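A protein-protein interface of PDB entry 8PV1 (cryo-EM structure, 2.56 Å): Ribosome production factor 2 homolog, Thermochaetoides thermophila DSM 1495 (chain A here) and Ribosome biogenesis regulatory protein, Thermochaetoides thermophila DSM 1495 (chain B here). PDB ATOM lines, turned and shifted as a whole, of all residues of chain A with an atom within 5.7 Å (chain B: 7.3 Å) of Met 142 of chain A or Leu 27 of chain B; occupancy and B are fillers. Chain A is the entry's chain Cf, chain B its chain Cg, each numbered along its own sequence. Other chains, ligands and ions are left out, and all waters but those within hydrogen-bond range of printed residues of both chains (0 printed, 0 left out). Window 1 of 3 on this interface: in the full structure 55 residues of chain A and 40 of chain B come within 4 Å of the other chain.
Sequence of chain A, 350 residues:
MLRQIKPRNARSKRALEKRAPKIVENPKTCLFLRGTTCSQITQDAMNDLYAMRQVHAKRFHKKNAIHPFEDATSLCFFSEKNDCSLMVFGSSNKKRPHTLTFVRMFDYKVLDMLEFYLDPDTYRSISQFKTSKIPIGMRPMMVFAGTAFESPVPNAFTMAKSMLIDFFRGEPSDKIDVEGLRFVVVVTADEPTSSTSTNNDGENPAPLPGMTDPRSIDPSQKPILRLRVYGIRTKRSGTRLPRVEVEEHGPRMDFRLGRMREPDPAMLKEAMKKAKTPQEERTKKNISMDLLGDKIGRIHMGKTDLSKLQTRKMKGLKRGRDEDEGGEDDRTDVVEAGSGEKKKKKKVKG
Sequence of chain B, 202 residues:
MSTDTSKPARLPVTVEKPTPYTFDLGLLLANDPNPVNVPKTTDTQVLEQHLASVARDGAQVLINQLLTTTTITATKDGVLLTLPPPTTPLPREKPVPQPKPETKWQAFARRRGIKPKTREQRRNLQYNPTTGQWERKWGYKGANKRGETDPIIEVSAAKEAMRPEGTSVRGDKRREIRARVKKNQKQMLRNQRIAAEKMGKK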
ATOM      1  N   ARG A 139     -13.149  -5.079  25.371  1.00  0.00           N
ATOM      2  CA  ARG A 139     -13.825  -5.096  24.081  1.00  0.00           C
ATOM      3  C   ARG A 139     -12.810  -4.962  22.949  1.00  0.00           C
ATOM      4  O   ARG A 139     -11.904  -4.130  23.023  1.00  0.00           O
ATOM      5  CB  ARG A 139     -14.834  -3.957  23.989  1.00  0.00           C
ATOM      6  CG  ARG A 139     -15.878  -3.956  25.080  1.00  0.00           C
ATOM      7  CD  ARG A 139     -16.863  -2.821  24.888  1.00  0.00           C
ATOM      8  NE  ARG A 139     -16.253  -1.509  25.072  1.00  0.00           N
ATOM      9  CZ  ARG A 139     -16.280  -0.536  24.171  1.00  0.00           C
ATOM     10  NH1 ARG A 139     -16.868  -0.697  22.998  1.00  0.00           N
ATOM     11  NH2 ARG A 139     -15.704   0.629  24.455  1.00  0.00           N
ATOM     12  N   PRO A 140     -12.930  -5.769  21.900  1.00  0.00           N
ATOM     13  CA  PRO A 140     -12.140  -5.538  20.691  1.00  0.00           C
ATOM     14  C   PRO A 140     -12.852  -4.578  19.749  1.00  0.00           C
ATOM     15  O   PRO A 140     -14.069  -4.391  19.806  1.00  0.00           O
ATOM     16  CB  PRO A 140     -12.045  -6.939  20.074  1.00  0.00           C
ATOM     17  CG  PRO A 140     -13.335  -7.577  20.461  1.00  0.00           C
ATOM     18  CD  PRO A 140     -13.725  -7.005  21.807  1.00  0.00           C
ATOM     19  N   MET A 141     -12.069  -3.959  18.875  1.00  0.00           N
ATOM     20  CA  MET A 141     -12.685  -3.180  17.813  1.00  0.00           C
ATOM     21  C   MET A 141     -13.057  -4.098  16.657  1.00  0.00           C
ATOM     22  O   MET A 141     -12.648  -5.256  16.603  1.00  0.00           O
ATOM     23  CB  MET A 141     -11.771  -2.053  17.341  1.00  0.00           C
ATOM     24  CG  MET A 141     -11.035  -1.343  18.457  1.00  0.00           C
ATOM     25  SD  MET A 141      -9.896  -0.097  17.834  1.00  0.00           S
ATOM     26  CE  MET A 141      -8.580  -1.119  17.215  1.00  0.00           C
ATOM     27  N   MET A 142     -13.869  -3.579  15.741  1.00  0.00           N
ATOM     28  CA  MET A 142     -14.458  -4.399  14.692  1.00  0.00           C
ATOM     29  C   MET A 142     -14.182  -3.799  13.324  1.00  0.00           C
ATOM     30  O   MET A 142     -14.282  -2.583  13.134  1.00  0.00           O
ATOM     31  CB  MET A 142     -15.969  -4.552  14.895  1.00  0.00           C
ATOM     32  CG  MET A 142     -16.352  -5.342  16.133  1.00  0.00           C
ATOM     33  SD  MET A 142     -18.134  -5.551  16.297  1.00  0.00           S
ATOM     34  CE  MET A 142     -18.621  -3.907  16.807  1.00  0.00           C
ATOM     35  N   VAL A 143     -13.833  -4.663  12.373  1.00  0.00           N
ATOM     36  CA  VAL A 143     -13.662  -4.294  10.974  1.00  0.00           C
ATOM     37  C   VAL A 143     -14.483  -5.265  10.138  1.00  0.00           C
ATOM     38  O   VAL A 143     -14.315  -6.484  10.258  1.00  0.00           O
ATOM     39  CB  VAL A 143     -12.186  -4.319  10.541  1.00  0.00           C
ATOM     40  CG1 VAL A 143     -12.069  -4.179   9.033  1.00  0.00           C
ATOM     41  CG2 VAL A 143     -11.405  -3.217  11.236  1.00  0.00           C
ATOM     42  N   PHE A 144     -15.380  -4.731   9.313  1.00  0.00           N
ATOM     43  CA  PHE A 144     -16.168  -5.519   8.372  1.00  0.00           C
ATOM     44  C   PHE A 144     -15.731  -5.131   6.965  1.00  0.00           C
ATOM     45  O   PHE A 144     -15.908  -3.981   6.550  1.00  0.00           O
ATOM     46  CB  PHE A 144     -17.663  -5.290   8.575  1.00  0.00           C
ATOM     47  CG  PHE A 144     -18.254  -6.103   9.689  1.00  0.00           C
ATOM     48  CD1 PHE A 144     -18.148  -5.682  11.002  1.00  0.00           C
ATOM     49  CD2 PHE A 144     -18.910  -7.291   9.424  1.00  0.00           C
ATOM     50  CE1 PHE A 144     -18.689  -6.425  12.031  1.00  0.00           C
ATOM     51  CE2 PHE A 144     -19.452  -8.042  10.449  1.00  0.00           C
ATOM     52  CZ  PHE A 144     -19.342  -7.607  11.754  1.00  0.00           C
ATOM     53  N   LEU A 164     -23.127 -10.294  14.262  1.00  0.00           N
ATOM     54  CA  LEU A 164     -21.766 -10.271  14.785  1.00  0.00           C
ATOM     55  C   LEU A 164     -21.449  -8.954  15.483  1.00  0.00           C
ATOM     56  O   LEU A 164     -20.692  -8.945  16.461  1.00  0.00           O
ATOM     57  CB  LEU A 164     -20.763 -10.540  13.665  1.00  0.00           C
ATOM     58  CG  LEU A 164     -20.763 -11.973  13.130  1.00  0.00           C
ATOM     59  CD1 LEU A 164     -19.856 -12.103  11.922  1.00  0.00           C
ATOM     60  CD2 LEU A 164     -20.351 -12.947  14.220  1.00  0.00           C
ATOM     61  N   ILE A 165     -22.014  -7.838  15.005  1.00  0.00           N
ATOM     62  CA  ILE A 165     -21.879  -6.575  15.726  1.00  0.00           C
ATOM     63  C   ILE A 165     -22.516  -6.682  17.106  1.00  0.00           C
ATOM     64  O   ILE A 165     -21.907  -6.305  18.114  1.00  0.00           O
ATOM     65  CB  ILE A 165     -22.486  -5.422  14.905  1.00  0.00           C
ATOM     66  CG1 ILE A 165     -21.551  -5.020  13.767  1.00  0.00           C
ATOM     67  CG2 ILE A 165     -22.769  -4.215  15.783  1.00  0.00           C
ATOM     68  CD1 ILE A 165     -22.203  -4.120  12.752  1.00  0.00           C
ATOM     69  N   PHE A 168     -20.210  -8.838  19.352  1.00  0.00           N
ATOM     70  CA  PHE A 168     -18.949  -8.245  19.782  1.00  0.00           C
ATOM     71  C   PHE A 168     -19.083  -6.802  20.260  1.00  0.00           C
ATOM     72  O   PHE A 168     -18.071  -6.099  20.338  1.00  0.00           O
ATOM     73  CB  PHE A 168     -17.916  -8.314  18.656  1.00  0.00           C
ATOM     74  CG  PHE A 168     -17.470  -9.705  18.321  1.00  0.00           C
ATOM     75  CD1 PHE A 168     -16.631 -10.402  19.173  1.00  0.00           C
ATOM     76  CD2 PHE A 168     -17.878 -10.314  17.148  1.00  0.00           C
ATOM     77  CE1 PHE A 168     -16.216 -11.681  18.866  1.00  0.00           C
ATOM     78  CE2 PHE A 168     -17.466 -11.593  16.835  1.00  0.00           C
ATOM     79  CZ  PHE A 168     -16.633 -12.278  17.696  1.00  0.00           C
ATOM     80  N   ARG A 169     -20.302  -6.334  20.551  1.00  0.00           N
ATOM     81  CA  ARG A 169     -20.461  -4.992  21.112  1.00  0.00           C
ATOM     82  C   ARG A 169     -19.801  -4.861  22.479  1.00  0.00           C
ATOM     83  O   ARG A 169     -19.076  -3.893  22.734  1.00  0.00           O
ATOM     84  CB  ARG A 169     -21.939  -4.624  21.231  1.00  0.00           C
ATOM     85  CG  ARG A 169     -22.505  -3.868  20.061  1.00  0.00           C
ATOM     86  CD  ARG A 169     -23.974  -3.598  20.273  1.00  0.00           C
ATOM     87  NE  ARG A 169     -24.188  -2.593  21.305  1.00  0.00           N
ATOM     88  CZ  ARG A 169     -25.380  -2.225  21.753  1.00  0.00           C
ATOM     89  NH1 ARG A 169     -26.490  -2.773  21.291  1.00  0.00           N
ATOM     90  NH2 ARG A 169     -25.458  -1.282  22.688  1.00  0.00           N
ATOM     91  N   PHE A 183      -6.863  -4.994  20.168  1.00  0.00           N
ATOM     92  CA  PHE A 183      -7.356  -6.198  19.513  1.00  0.00           C
ATOM     93  C   PHE A 183      -8.472  -5.853  18.539  1.00  0.00           C
ATOM     94  O   PHE A 183      -9.328  -5.012  18.830  1.00  0.00           O
ATOM     95  CB  PHE A 183      -7.846  -7.230  20.538  1.00  0.00           C
ATOM     96  CG  PHE A 183      -6.754  -7.778  21.407  1.00  0.00           C
ATOM     97  CD1 PHE A 183      -5.968  -8.830  20.969  1.00  0.00           C
ATOM     98  CD2 PHE A 183      -6.507  -7.242  22.660  1.00  0.00           C
ATOM     99  CE1 PHE A 183      -4.958  -9.335  21.758  1.00  0.00           C
ATOM    100  CE2 PHE A 183      -5.498  -7.746  23.456  1.00  0.00           C
ATOM    101  CZ  PHE A 183      -4.722  -8.793  23.003  1.00  0.00           C
ATOM    102  N   VAL A 184      -8.462  -6.518  17.385  1.00  0.00           N
ATOM    103  CA  VAL A 184      -9.398  -6.230  16.306  1.00  0.00           C
ATOM    104  C   VAL A 184      -9.981  -7.539  15.778  1.00  0.00           C
ATOM    105  O   VAL A 184      -9.261  -8.519  15.558  1.00  0.00           O
ATOM    106  CB  VAL A 184      -8.726  -5.397  15.188  1.00  0.00           C
ATOM    107  CG1 VAL A 184      -7.452  -6.062  14.675  1.00  0.00           C
ATOM    108  CG2 VAL A 184      -9.693  -5.120  14.049  1.00  0.00           C
ATOM    109  N   VAL A 185     -11.299  -7.559  15.612  1.00  0.00           N
ATOM    110  CA  VAL A 185     -12.021  -8.677  15.024  1.00  0.00           C
ATOM    111  C   VAL A 185     -12.429  -8.282  13.614  1.00  0.00           C
ATOM    112  O   VAL A 185     -13.125  -7.277  13.421  1.00  0.00           O
ATOM    113  CB  VAL A 185     -13.250  -9.045  15.872  1.00  0.00           C
ATOM    114  CG1 VAL A 185     -14.109 -10.048  15.149  1.00  0.00           C
ATOM    115  CG2 VAL A 185     -12.817  -9.592  17.220  1.00  0.00           C
ATOM    116  N   VAL A 186     -11.995  -9.061  12.628  1.00  0.00           N
ATOM    117  CA  VAL A 186     -12.190  -8.739  11.222  1.00  0.00           C
ATOM    118  C   VAL A 186     -13.069  -9.812  10.596  1.00  0.00           C
ATOM    119  O   VAL A 186     -12.756 -11.008  10.671  1.00  0.00           O
ATOM    120  CB  VAL A 186     -10.852  -8.621  10.475  1.00  0.00           C
ATOM    121  CG1 VAL A 186     -11.084  -8.181   9.039  1.00  0.00           C
ATOM    122  CG2 VAL A 186      -9.942  -7.643  11.189  1.00  0.00           C
ATOM    123  N   ASP B  24     -18.039   4.029  12.775  1.00  0.00           N
ATOM    124  CA  ASP B  24     -18.969   4.198  13.893  1.00  0.00           C
ATOM    125  C   ASP B  24     -18.094   4.065  15.141  1.00  0.00           C
ATOM    126  O   ASP B  24     -17.840   2.968  15.639  1.00  0.00           O
ATOM    127  CB  ASP B  24     -20.103   3.174  13.865  1.00  0.00           C
ATOM    128  CG  ASP B  24     -21.236   3.525  14.817  1.00  0.00           C
ATOM    129  OD1 ASP B  24     -21.060   4.413  15.676  1.00  0.00           O
ATOM    130  OD2 ASP B  24     -22.313   2.910  14.704  1.00  0.00           O
ATOM    131  N   LEU B  25     -17.611   5.204  15.635  1.00  0.00           N
ATOM    132  CA  LEU B  25     -16.636   5.179  16.718  1.00  0.00           C
ATOM    133  C   LEU B  25     -17.269   4.859  18.064  1.00  0.00           C
ATOM    134  O   LEU B  25     -16.544   4.576  19.024  1.00  0.00           O
ATOM    135  CB  LEU B  25     -15.891   6.513  16.769  1.00  0.00           C
ATOM    136  CG  LEU B  25     -15.168   6.874  15.469  1.00  0.00           C
ATOM    137  CD1 LEU B  25     -14.321   8.118  15.641  1.00  0.00           C
ATOM    138  CD2 LEU B  25     -14.312   5.714  14.977  1.00  0.00           C
ATOM    139  N   GLY B  26     -18.599   4.902  18.160  1.00  0.00           N
ATOM    140  CA  GLY B  26     -19.258   4.445  19.371  1.00  0.00           C
ATOM    141  C   GLY B  26     -19.112   2.953  19.594  1.00  0.00           C
ATOM    142  O   GLY B  26     -18.949   2.504  20.732  1.00  0.00           O
ATOM    143  N   LEU B  27     -19.168   2.168  18.521  1.00  0.00           N
ATOM    144  CA  LEU B  27     -18.979   0.726  18.586  1.00  0.00           C
ATOM    145  C   LEU B  27     -17.566   0.305  18.210  1.00  0.00           C
ATOM    146  O   LEU B  27     -17.294  -0.899  18.140  1.00  0.00           O
ATOM    147  CB  LEU B  27     -19.984   0.019  17.676  1.00  0.00           C
ATOM    148  CG  LEU B  27     -21.468   0.247  17.952  1.00  0.00           C
ATOM    149  CD1 LEU B  27     -22.305  -0.475  16.914  1.00  0.00           C
ATOM    150  CD2 LEU B  27     -21.829  -0.218  19.350  1.00  0.00           C
ATOM    151  N   LEU B  28     -16.669   1.271  17.972  1.00  0.00           N
ATOM    152  CA  LEU B  28     -15.311   1.033  17.467  1.00  0.00           C
ATOM    153  C   LEU B  28     -15.336   0.223  16.174  1.00  0.00           C
ATOM    154  O   LEU B  28     -14.541  -0.698  15.975  1.00  0.00           O
ATOM    155  CB  LEU B  28     -14.431   0.353  18.518  1.00  0.00           C
ATOM    156  CG  LEU B  28     -14.385   0.975  19.911  1.00  0.00           C
ATOM    157  CD1 LEU B  28     -13.769  -0.002  20.893  1.00  0.00           C
ATOM    158  CD2 LEU B  28     -13.604   2.274  19.885  1.00  0.00           C
ATOM    159  N   LEU B  29     -16.259   0.572  15.283  1.00  0.00           N
ATOM    160  CA  LEU B  29     -16.544  -0.204  14.086  1.00  0.00           C
ATOM    161  C   LEU B  29     -16.029   0.526  12.854  1.00  0.00           C
ATOM    162  O   LEU B  29     -16.296   1.718  12.677  1.00  0.00           O
ATOM    163  CB  LEU B  29     -18.047  -0.456  13.960  1.00  0.00           C
ATOM    164  CG  LEU B  29     -18.544  -1.058  12.651  1.00  0.00           C
ATOM    165  CD1 LEU B  29     -17.977  -2.449  12.483  1.00  0.00           C
ATOM    166  CD2 LEU B  29     -20.057  -1.079  12.623  1.00  0.00           C
ATOM    167  N   ALA B  30     -15.295  -0.193  12.011  1.00  0.00           N
ATOM    168  CA  ALA B  30     -14.837   0.309  10.723  1.00  0.00           C
ATOM    169  C   ALA B  30     -15.442  -0.550   9.625  1.00  0.00           C
ATOM    170  O   ALA B  30     -15.396  -1.780   9.704  1.00  0.00           O
ATOM    171  CB  ALA B  30     -13.310   0.293  10.631  1.00  0.00           C
ATOM    172  N   ASN B  31     -16.014   0.092   8.609  1.00  0.00           N
ATOM    173  CA  ASN B  31     -16.628  -0.605   7.485  1.00  0.00           C
ATOM    174  C   ASN B  31     -15.825  -0.309   6.227  1.00  0.00           C
ATOM    175  O   ASN B  31     -15.630   0.860   5.864  1.00  0.00           O
ATOM    176  CB  ASN B  31     -18.086  -0.194   7.309  1.00  0.00           C
ATOM    177  CG  ASN B  31     -18.873  -0.266   8.596  1.00  0.00           C
ATOM    178  OD1 ASN B  31     -18.998   0.722   9.317  1.00  0.00           O
ATOM    179  ND2 ASN B  31     -19.407  -1.441   8.895  1.00  0.00           N
ATOM    180  N   GLY B  58      -7.466  -1.915   7.906  1.00  0.00           N
ATOM    181  CA  GLY B  58      -8.617  -1.501   8.696  1.00  0.00           C
ATOM    182  C   GLY B  58      -8.238  -0.994  10.075  1.00  0.00           C
ATOM    183  O   GLY B  58      -8.768   0.020  10.543  1.00  0.00           O
ATOM    184  N   LEU B  62      -8.740   2.844  11.435  1.00  0.00           N
ATOM    185  CA  LEU B  62      -9.512   3.004  12.665  1.00  0.00           C
ATOM    186  C   LEU B  62      -8.717   3.753  13.731  1.00  0.00           C
ATOM    187  O   LEU B  62      -9.251   4.638  14.412  1.00  0.00           O
ATOM    188  CB  LEU B  62      -9.957   1.636  13.178  1.00  0.00           C
ATOM    189  CG  LEU B  62     -11.120   1.626  14.166  1.00  0.00           C
ATOM    190  CD1 LEU B  62     -12.303   2.392  13.615  1.00  0.00           C
ATOM    191  CD2 LEU B  62     -11.513   0.199  14.460  1.00  0.00           C
ATOM    192  N   LEU B  83     -15.988   9.259  22.956  1.00  0.00           N
ATOM    193  CA  LEU B  83     -16.609   8.633  21.798  1.00  0.00           C
ATOM    194  C   LEU B  83     -17.995   9.207  21.545  1.00  0.00           C
ATOM    195  O   LEU B  83     -18.699   9.579  22.491  1.00  0.00           O
ATOM    196  CB  LEU B  83     -16.729   7.122  22.001  1.00  0.00           C
ATOM    197  CG  LEU B  83     -15.450   6.332  22.270  1.00  0.00           C
ATOM    198  CD1 LEU B  83     -15.801   4.910  22.669  1.00  0.00           C
ATOM    199  CD2 LEU B  83     -14.543   6.347  21.056  1.00  0.00           C
ATOM    200  N   PRO B  84     -18.406   9.289  20.277  1.00  0.00           N
ATOM    201  CA  PRO B  84     -19.789   9.646  19.984  1.00  0.00           C
ATOM    202  C   PRO B  84     -20.718   8.501  20.339  1.00  0.00           C
ATOM    203  O   PRO B  84     -20.274   7.351  20.498  1.00  0.00           O
ATOM    204  CB  PRO B  84     -19.772   9.906  18.466  1.00  0.00           C
ATOM    205  CG  PRO B  84     -18.633   9.093  17.971  1.00  0.00           C
ATOM    206  CD  PRO B  84     -17.598   9.153  19.052  1.00  0.00           C
ATOM    207  N   PRO B  85     -22.011   8.769  20.510  1.00  0.00           N
ATOM    208  CA  PRO B  85     -22.979   7.679  20.694  1.00  0.00           C
ATOM    209  C   PRO B  85     -23.054   6.807  19.454  1.00  0.00           C
ATOM    210  O   PRO B  85     -22.813   7.290  18.336  1.00  0.00           O
ATOM    211  CB  PRO B  85     -24.304   8.417  20.942  1.00  0.00           C
ATOM    212  CG  PRO B  85     -24.085   9.794  20.419  1.00  0.00           C
ATOM    213  CD  PRO B  85     -22.643  10.089  20.662  1.00  0.00           C
ATOM    214  N   PRO B  86     -23.346   5.514  19.614  1.00  0.00           N
ATOM    215  CA  PRO B  86     -23.384   4.613  18.455  1.00  0.00           C
ATOM    216  C   PRO B  86     -24.488   4.980  17.475  1.00  0.00           C
ATOM    217  O   PRO B  86     -25.582   5.392  17.866  1.00  0.00           O
ATOM    218  CB  PRO B  86     -23.630   3.237  19.087  1.00  0.00           C
ATOM    219  CG  PRO B  86     -23.176   3.383  20.501  1.00  0.00           C
ATOM    220  CD  PRO B  86     -23.518   4.786  20.880  1.00  0.00           C
ATOM    221  N   THR B  87     -24.188   4.823  16.187  1.00  0.00           N
ATOM    222  CA  THR B  87     -25.113   5.174  15.118  1.00  0.00           C
ATOM    223  C   THR B  87     -25.578   3.987  14.293  1.00  0.00           C
ATOM    224  O   THR B  87     -26.485   4.144  13.474  1.00  0.00           O
ATOM    225  CB  THR B  87     -24.477   6.203  14.176  1.00  0.00           C
ATOM    226  OG1 THR B  87     -23.317   5.634  13.557  1.00  0.00           O
ATOM    227  CG2 THR B  87     -24.073   7.452  14.943  1.00  0.00           C
ATOM    228  N   THR B  88     -24.977   2.815  14.474  1.00  0.00           N
ATOM    229  CA  THR B  88     -25.399   1.627  13.745  1.00  0.00           C
ATOM    230  C   THR B  88     -26.767   1.178  14.242  1.00  0.00           C
ATOM    231  O   THR B  88     -26.949   1.000  15.456  1.00  0.00           O
ATOM    232  CB  THR B  88     -24.386   0.498  13.908  1.00  0.00           C
ATOM    233  OG1 THR B  88     -23.119   0.914  13.385  1.00  0.00           O
ATOM    234  CG2 THR B  88     -24.845  -0.744  13.164  1.00  0.00           C
ATOM    235  N   PRO B  89     -27.749   1.001  13.359  1.00  0.00           N
ATOM    236  CA  PRO B  89     -29.081   0.575  13.808  1.00  0.00           C
ATOM    237  C   PRO B  89     -29.066  -0.880  14.257  1.00  0.00           C
ATOM    238  O   PRO B  89     -28.754  -1.781  13.476  1.00  0.00           O
ATOM    239  CB  PRO B  89     -29.955   0.777  12.564  1.00  0.00           C
ATOM    240  CG  PRO B  89     -29.152   1.656  11.650  1.00  0.00           C
ATOM    241  CD  PRO B  89     -27.730   1.307  11.921  1.00  0.00           C
ATOM    242  N   LEU B  90     -29.408  -1.102  15.522  1.00  0.00           N
ATOM    243  CA  LEU B  90     -29.372  -2.422  16.130  1.00  0.00           C
ATOM    244  C   LEU B  90     -30.665  -2.669  16.889  1.00  0.00           C
ATOM    245  O   LEU B  90     -31.225  -1.741  17.484  1.00  0.00           O
ATOM    246  CB  LEU B  90     -28.175  -2.563  17.082  1.00  0.00           C
ATOM    247  CG  LEU B  90     -26.813  -2.686  16.401  1.00  0.00           C
ATOM    248  CD1 LEU B  90     -25.711  -2.245  17.339  1.00  0.00           C
ATOM    249  CD2 LEU B  90     -26.578  -4.112  15.936  1.00  0.00           C
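N of Met 142 of chain A is in hydrogen-bond range of O of Leu 28 of chain B (3.0 Å).
O of Met 142 of chain A sits at hydrogen-bond distance from N of Ala 30 of chain B (2.8 Å).
N of Phe 144 of chain A lies within hydrogen-bond range of O of Ala 30 of chain B.
The backbone carbonyl oxygen (O) of Phe 183 of chain A is in hydrogen-bond range of the backbone NH (N) of Met 141 of chain A.
The backbone carbonyl oxygen (O) of Met 141 of chain A is in hydrogen-bond range of the backbone NH (N) of Val 185 of chain A (2.8 Å).
N of Val 143 of chain A lies within hydrogen-bond range of O of Val 185 of chain A, 2.9 Å away.
The backbone NH (N) of Leu 29 of chain B sits at hydrogen-bond distance from the backbone carbonyl oxygen (O) of Asp 24 of chain B (2.9 Å).
Among the printed residues, pairs that only touch across the chains: Val 143 of chain A with Ala 30 of chain B, Met 141 of chain A with Leu 28 of chain B, Met 142 of chain A with Leu 29 of chain B, Met 142 of chain A with Leu 27 of chain B, Phe 144 of chain A with Leu 29 of chain B, Phe 144 of chain A with Asn 31 of chain B, Met 141 of chain A with Leu 62 of chain B, Arg 169 of chain A with Leu 90 of chain B, Ile 165 of chain A with Leu 29 of chain B, Arg 169 of chain A with Leu 27 of chain B, Arg 139 of chain A with Leu 28 of chain B, Ile 165 of chain A with Leu 90 of chain B and Ile 165 of chain A with Leu 27 of chain B.
Of the printed residues of chain B, Met 142 of chain A touches Leu 27, Leu 28, Leu 29 and Ala 30.
Printed residues of chain A within 4 Å of Leu 27 of chain B: Met 142, Ile 165 and Arg 169.
Of the printed residues of chain A, Leu 62 of chain B touches Met 141 (3.7 Å).
Of the printed residues of chain B, Met 141 of chain A touches Leu 28 and Leu 62.
Printed residues of chain A within 4 Å of Asn 31 of chain B: Phe 144.
Of the printed residues of chain B, Phe 144 of chain A touches Leu 29, Ala 30 and Asn 31.
Of the printed residues of chain A, Leu 28 of chain B touches Arg 139 (3.8 Å), Met 141 (3.4 Å) and Met 142 (3.0 Å).
Pro 140 of chain A touches none of the printed residues of chain B.
Leu 164 of chain A touches none of the printed residues of chain B.
The nearest residue of chain B that does not touch Met 142 of chain A is Leu 62 of chain B (4.1 Å).
The nearest residue of chain A that does not touch Leu 27 of chain B is Arg 139 of chain A (4.9 Å).
Of the 18 printed residues of chain B, 7 touch a printed residue of chain A.
Printed residues of chain B that touch a printed residue of chain A: Leu 27, Leu 28, Leu 29, Ala 30, Asn 31, Leu 62 and Leu 90.
Of the 14 printed residues of chain A, 7 touch a printed residue of chain B.
Hydrophobic or aromatic side chains of chain A that line the printed part of chain B: Met 141, Met 142, Phe 144 and Ile 165.
Among the printed residues, 16 pairs touch across the chains.
Among the printed residues, no Asp or Glu carboxylate lies within 4 Å of a Lys or Arg side-chain nitrogen of the other chain.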
